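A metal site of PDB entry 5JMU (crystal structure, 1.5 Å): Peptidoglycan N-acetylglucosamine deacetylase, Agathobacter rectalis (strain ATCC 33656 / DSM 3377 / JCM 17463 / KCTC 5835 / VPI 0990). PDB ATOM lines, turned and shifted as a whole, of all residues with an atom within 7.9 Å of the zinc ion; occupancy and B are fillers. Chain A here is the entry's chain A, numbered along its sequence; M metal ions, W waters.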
ATOM      1  N   PHE A  26      36.233 -24.157  -1.291  1.00  0.00           N
ATOM      2  CA  PHE A  26      35.589 -25.444  -1.582  1.00  0.00           C
ATOM      3  C   PHE A  26      34.248 -25.542  -0.847  1.00  0.00           C
ATOM      4  O   PHE A  26      34.229 -25.496   0.411  1.00  0.00           O
ATOM      5  CB  PHE A  26      36.514 -26.607  -1.172  1.00  0.00           C
ATOM      6  CG  PHE A  26      37.841 -26.582  -1.923  1.00  0.00           C
ATOM      7  CD1 PHE A  26      37.919 -27.148  -3.204  1.00  0.00           C
ATOM      8  CD2 PHE A  26      38.956 -25.955  -1.370  1.00  0.00           C
ATOM      9  CE1 PHE A  26      39.107 -27.091  -3.962  1.00  0.00           C
ATOM     10  CE2 PHE A  26      40.163 -25.893  -2.087  1.00  0.00           C
ATOM     11  CZ  PHE A  26      40.236 -26.462  -3.398  1.00  0.00           C
ATOM     12  N   ASP A  27      33.187 -25.780  -1.623  1.00  0.00           N
ATOM     13  CA  ASP A  27      31.822 -25.902  -1.061  1.00  0.00           C
ATOM     14  C   ASP A  27      31.379 -27.318  -1.015  1.00  0.00           C
ATOM     15  O   ASP A  27      31.811 -28.144  -1.827  1.00  0.00           O
ATOM     16  CB  ASP A  27      30.748 -25.205  -1.930  1.00  0.00           C
ATOM     17  CG  ASP A  27      30.698 -23.696  -1.752  1.00  0.00           C
ATOM     18  OD1 ASP A  27      31.587 -23.110  -1.106  1.00  0.00           O
ATOM     19  OD2 ASP A  27      29.743 -23.137  -2.337  1.00  0.00           O
ATOM     20  N   ASP A  28      30.464 -27.552  -0.081  1.00  0.00           N
ATOM     21  CA  ASP A  28      29.563 -28.727  -0.050  1.00  0.00           C
ATOM     22  C   ASP A  28      30.120 -29.933   0.694  1.00  0.00           C
ATOM     23  O   ASP A  28      29.362 -30.829   1.009  1.00  0.00           O
ATOM     24  CB  ASP A  28      29.136 -29.183  -1.468  1.00  0.00           C
ATOM     25  CG  ASP A  28      28.043 -28.337  -2.073  1.00  0.00           C
ATOM     26  OD1 ASP A  28      27.835 -27.168  -1.642  1.00  0.00           O
ATOM     27  OD2 ASP A  28      27.479 -28.766  -3.088  1.00  0.00           O
ATOM     28  N   GLY A  29      31.436 -29.965   0.973  1.00  0.00           N
ATOM     29  CA  GLY A  29      32.036 -31.039   1.721  1.00  0.00           C
ATOM     30  C   GLY A  29      31.817 -30.882   3.218  1.00  0.00           C
ATOM     31  O   GLY A  29      31.120 -29.964   3.630  1.00  0.00           O
ATOM     32  N   PHE A  51      33.853 -24.242   2.851  1.00  0.00           N
ATOM     33  CA  PHE A  51      32.487 -23.851   3.237  1.00  0.00           C
ATOM     34  C   PHE A  51      31.692 -25.145   3.393  1.00  0.00           C
ATOM     35  O   PHE A  51      31.294 -25.747   2.387  1.00  0.00           O
ATOM     36  CB  PHE A  51      31.891 -22.898   2.192  1.00  0.00           C
ATOM     37  CG  PHE A  51      32.573 -21.559   2.174  1.00  0.00           C
ATOM     38  CD1 PHE A  51      32.190 -20.591   3.095  1.00  0.00           C
ATOM     39  CD2 PHE A  51      33.576 -21.279   1.270  1.00  0.00           C
ATOM     40  CE1 PHE A  51      32.778 -19.328   3.081  1.00  0.00           C
ATOM     41  CE2 PHE A  51      34.192 -20.019   1.259  1.00  0.00           C
ATOM     42  CZ  PHE A  51      33.784 -19.022   2.167  1.00  0.00           C
ATOM     43  N   THR A  53      29.214 -28.469   5.016  1.00  0.00           N
ATOM     44  CA  THR A  53      27.846 -28.901   5.204  1.00  0.00           C
ATOM     45  C   THR A  53      27.876 -30.141   6.069  1.00  0.00           C
ATOM     46  O   THR A  53      28.967 -30.689   6.313  1.00  0.00           O
ATOM     47  CB  THR A  53      27.151 -29.322   3.880  1.00  0.00           C
ATOM     48  OG1 THR A  53      27.732 -30.564   3.417  1.00  0.00           O
ATOM     49  CG2 THR A  53      27.247 -28.252   2.818  1.00  0.00           C
ATOM     50  N   HIS A  76      28.574 -23.347   5.173  1.00  0.00           N
ATOM     51  CA  HIS A  76      27.757 -23.310   3.946  1.00  0.00           C
ATOM     52  C   HIS A  76      26.304 -23.563   4.373  1.00  0.00           C
ATOM     53  O   HIS A  76      25.456 -22.658   4.334  1.00  0.00           O
ATOM     54  CB  HIS A  76      28.279 -24.325   2.932  1.00  0.00           C
ATOM     55  CG  HIS A  76      27.753 -24.176   1.524  1.00  0.00           C
ATOM     56  ND1 HIS A  76      27.484 -22.948   0.943  1.00  0.00           N
ATOM     57  CD2 HIS A  76      27.512 -25.126   0.583  1.00  0.00           C
ATOM     58  CE1 HIS A  76      27.063 -23.166  -0.308  1.00  0.00           C
ATOM     59  NE2 HIS A  76      27.054 -24.475  -0.544  1.00  0.00           N
ATOM     60  N   SER A  77      26.047 -24.751   4.885  1.00  0.00           N
ATOM     61  CA  SER A  77      24.707 -25.082   5.388  1.00  0.00           C
ATOM     62  C   SER A  77      24.713 -26.479   5.991  1.00  0.00           C
ATOM     63  O   SER A  77      25.380 -27.355   5.476  1.00  0.00           O
ATOM     64  CB  SER A  77      23.679 -25.027   4.233  1.00  0.00           C
ATOM     65  OG  SER A  77      22.454 -25.614   4.647  1.00  0.00           O
ATOM     66  N   HIS A  80      21.907 -28.137   3.528  1.00  0.00           N
ATOM     67  CA  HIS A  80      22.028 -27.747   2.127  1.00  0.00           C
ATOM     68  C   HIS A  80      20.735 -28.060   1.371  1.00  0.00           C
ATOM     69  O   HIS A  80      20.770 -28.478   0.204  1.00  0.00           O
ATOM     70  CB  HIS A  80      23.224 -28.460   1.474  1.00  0.00           C
ATOM     71  CG  HIS A  80      23.762 -27.771   0.253  1.00  0.00           C
ATOM     72  ND1 HIS A  80      23.294 -28.035  -1.015  1.00  0.00           N
ATOM     73  CD2 HIS A  80      24.757 -26.864   0.114  1.00  0.00           C
ATOM     74  CE1 HIS A  80      23.959 -27.302  -1.893  1.00  0.00           C
ATOM     75  NE2 HIS A  80      24.855 -26.585  -1.244  1.00  0.00           N
ATOM     76  N   TYR A  82      17.665 -26.205  -0.076  1.00  0.00           N
ATOM     77  CA  TYR A  82      17.157 -24.864  -0.366  1.00  0.00           C
ATOM     78  C   TYR A  82      15.719 -24.721   0.123  1.00  0.00           C
ATOM     79  O   TYR A  82      15.333 -23.671   0.657  1.00  0.00           O
ATOM     80  CB  TYR A  82      17.226 -24.518  -1.902  1.00  0.00           C
ATOM     81  CG  TYR A  82      18.629 -24.525  -2.487  1.00  0.00           C
ATOM     82  CD1 TYR A  82      19.556 -23.557  -2.148  1.00  0.00           C
ATOM     83  CD2 TYR A  82      19.042 -25.522  -3.374  1.00  0.00           C
ATOM     84  CE1 TYR A  82      20.865 -23.585  -2.665  1.00  0.00           C
ATOM     85  CE2 TYR A  82      20.367 -25.539  -3.894  1.00  0.00           C
ATOM     86  CZ  TYR A  82      21.272 -24.568  -3.536  1.00  0.00           C
ATOM     87  OH  TYR A  82      22.587 -24.572  -4.007  1.00  0.00           O
ATOM     88  N   ARG A 115      29.110 -18.875   3.427  1.00  0.00           N
ATOM     89  CA  ARG A 115      28.759 -18.688   2.022  1.00  0.00           C
ATOM     90  C   ARG A 115      27.328 -19.164   1.870  1.00  0.00           C
ATOM     91  O   ARG A 115      27.037 -20.337   2.129  1.00  0.00           O
ATOM     92  CB  ARG A 115      29.684 -19.468   1.094  1.00  0.00           C
ATOM     93  CG  ARG A 115      29.181 -19.380  -0.408  1.00  0.00           C
ATOM     94  CD  ARG A 115      30.246 -19.980  -1.314  1.00  0.00           C
ATOM     95  NE  ARG A 115      31.395 -19.094  -1.450  1.00  0.00           N
ATOM     96  CZ  ARG A 115      32.618 -19.539  -1.809  1.00  0.00           C
ATOM     97  NH1 ARG A 115      32.814 -20.843  -2.017  1.00  0.00           N
ATOM     98  NH2 ARG A 115      33.638 -18.679  -1.982  1.00  0.00           N
ATOM     99  N   PHE A 116      26.453 -18.289   1.423  1.00  0.00           N
ATOM    100  CA  PHE A 116      25.074 -18.664   1.213  1.00  0.00           C
ATOM    101  C   PHE A 116      24.966 -19.735   0.142  1.00  0.00           C
ATOM    102  O   PHE A 116      25.607 -19.613  -0.909  1.00  0.00           O
ATOM    103  CB  PHE A 116      24.258 -17.464   0.740  1.00  0.00           C
ATOM    104  CG  PHE A 116      24.048 -16.406   1.761  1.00  0.00           C
ATOM    105  CD1 PHE A 116      23.079 -16.538   2.782  1.00  0.00           C
ATOM    106  CD2 PHE A 116      24.819 -15.244   1.730  1.00  0.00           C
ATOM    107  CE1 PHE A 116      22.851 -15.521   3.711  1.00  0.00           C
ATOM    108  CE2 PHE A 116      24.610 -14.207   2.695  1.00  0.00           C
ATOM    109  CZ  PHE A 116      23.637 -14.340   3.694  1.00  0.00           C
ATOM    110  N   PRO A 117      24.128 -20.775   0.370  1.00  0.00           N
ATOM    111  CA  PRO A 117      23.877 -21.723  -0.711  1.00  0.00           C
ATOM    112  C   PRO A 117      23.267 -21.010  -1.911  1.00  0.00           C
ATOM    113  O   PRO A 117      22.322 -20.232  -1.798  1.00  0.00           O
ATOM    114  CB  PRO A 117      22.934 -22.751  -0.052  1.00  0.00           C
ATOM    115  CG  PRO A 117      23.420 -22.754   1.427  1.00  0.00           C
ATOM    116  CD  PRO A 117      23.638 -21.273   1.690  1.00  0.00           C
ATOM    117  N   GLY A 118      23.872 -21.239  -3.075  1.00  0.00           N
ATOM    118  CA  GLY A 118      23.481 -20.582  -4.320  1.00  0.00           C
ATOM    119  C   GLY A 118      24.158 -19.214  -4.488  1.00  0.00           C
ATOM    120  O   GLY A 118      23.950 -18.546  -5.515  1.00  0.00           O
ATOM    121  N   GLY A 119      24.950 -18.798  -3.501  1.00  0.00           N
ATOM    122  CA  GLY A 119      25.531 -17.446  -3.485  1.00  0.00           C
ATOM    123  C   GLY A 119      24.552 -16.426  -2.887  1.00  0.00           C
ATOM    124  O   GLY A 119      23.342 -16.694  -2.853  1.00  0.00           O
ATOM    125  N   LEU A 184      35.580 -20.597  -6.839  1.00  0.00           N
ATOM    126  CA  LEU A 184      34.609 -21.560  -6.357  1.00  0.00           C
ATOM    127  C   LEU A 184      34.847 -22.936  -6.921  1.00  0.00           C
ATOM    128  O   LEU A 184      34.748 -23.116  -8.132  1.00  0.00           O
ATOM    129  CB  LEU A 184      33.167 -21.134  -6.749  1.00  0.00           C
ATOM    130  CG  LEU A 184      32.001 -22.100  -6.509  1.00  0.00           C
ATOM    131  CD1 LEU A 184      31.862 -22.350  -4.970  1.00  0.00           C
ATOM    132  CD2 LEU A 184      30.709 -21.512  -7.043  1.00  0.00           C
ATOM    133  N   GLN A 185      35.172 -23.914  -6.081  1.00  0.00           N
ATOM    134  CA  GLN A 185      35.134 -25.326  -6.439  1.00  0.00           C
ATOM    135  C   GLN A 185      34.324 -26.079  -5.387  1.00  0.00           C
ATOM    136  O   GLN A 185      33.956 -25.523  -4.340  1.00  0.00           O
ATOM    137  CB  GLN A 185      36.529 -25.955  -6.539  1.00  0.00           C
ATOM    138  CG  GLN A 185      37.358 -25.441  -7.712  1.00  0.00           C
ATOM    139  CD  GLN A 185      38.771 -25.996  -7.668  1.00  0.00           C
ATOM    140  OE1 GLN A 185      39.702 -25.362  -7.124  1.00  0.00           O
ATOM    141  NE2 GLN A 185      38.948 -27.214  -8.221  1.00  0.00           N
ATOM    142  N   HIS A 186      34.071 -27.359  -5.655  1.00  0.00           N
ATOM    143  CA  HIS A 186      33.321 -28.189  -4.742  1.00  0.00           C
ATOM    144  C   HIS A 186      34.162 -29.409  -4.432  1.00  0.00           C
ATOM    145  O   HIS A 186      34.443 -30.201  -5.349  1.00  0.00           O
ATOM    146  CB  HIS A 186      31.986 -28.615  -5.392  1.00  0.00           C
ATOM    147  CG  HIS A 186      31.027 -27.470  -5.582  1.00  0.00           C
ATOM    148  ND1 HIS A 186      31.175 -26.546  -6.608  1.00  0.00           N
ATOM    149  CD2 HIS A 186      29.920 -27.092  -4.892  1.00  0.00           C
ATOM    150  CE1 HIS A 186      30.189 -25.654  -6.529  1.00  0.00           C
ATOM    151  NE2 HIS A 186      29.415 -25.966  -5.507  1.00  0.00           N
ATOM    152  N   ILE A 188      33.381 -32.105  -3.081  1.00  0.00           N
ATOM    153  CA  ILE A 188      32.646 -33.349  -3.252  1.00  0.00           C
ATOM    154  C   ILE A 188      32.706 -33.876  -4.698  1.00  0.00           C
ATOM    155  O   ILE A 188      32.169 -34.960  -4.977  1.00  0.00           O
ATOM    156  CB  ILE A 188      31.169 -33.184  -2.859  1.00  0.00           C
ATOM    157  CG1 ILE A 188      30.551 -32.022  -3.621  1.00  0.00           C
ATOM    158  CG2 ILE A 188      31.055 -33.025  -1.338  1.00  0.00           C
ATOM    159  CD1 ILE A 188      29.011 -32.104  -3.661  1.00  0.00           C
HETATM  160 ZN    ZN M   1      26.526 -25.607  -2.231  1.00  0.00          ZN
HETATM  161  O   HOH W   1      25.173 -24.084  -2.957  1.00  0.00           O
HETATM  162  O   HOH W   2      27.973 -24.704  -3.379  1.00  0.00           O
HETATM  163  O   HOH W   3      26.091 -26.670  -4.004  1.00  0.00           O
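N of Asp 28 lies within hydrogen-bond range of O of Phe 51 (3.2 Å). A ring nitrogen (NE2) of His 76 sits close to the side-chain carboxylate of Asp 27 (3.5 Å). The side-chain hydroxyl (OG1) of Thr 53 lies within hydrogen-bond range of the backbone carbonyl oxygen (O) of Asp 28 (2.9 Å). The backbone carbonyl oxygen (O) of Arg 115 is in hydrogen-bond range of a ring nitrogen (ND1) of His 76 (2.9 Å). The backbone NH (N) of His 80 sits at hydrogen-bond distance from the side-chain hydroxyl (OG) of Ser 77.
Three residues have an atom within 4 Å of the zinc ion: Asp 28, His 76 and His 80.
The zinc ion is bound by water W2 (2.1 Å). NE2 of His 76 is bound to the zinc ion (2.1 Å). The zinc ion is bound by water W3 (2.1 Å). The zinc ion is bound by the side-chain carboxylate (OD1) of Asp 28 (2.1 Å). Water W1 is bound to the zinc ion, 2.2 Å away. NE2 of His 80 is bound to the zinc ion (2.2 Å). The zinc ion has six donor atoms within binding distance.
Water W2 lies within hydrogen-bond range of OD2 of Asp 27 and NE2 of His 186. Water W1 lies within hydrogen-bond range of OH of Tyr 82 and N of Gly 118.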
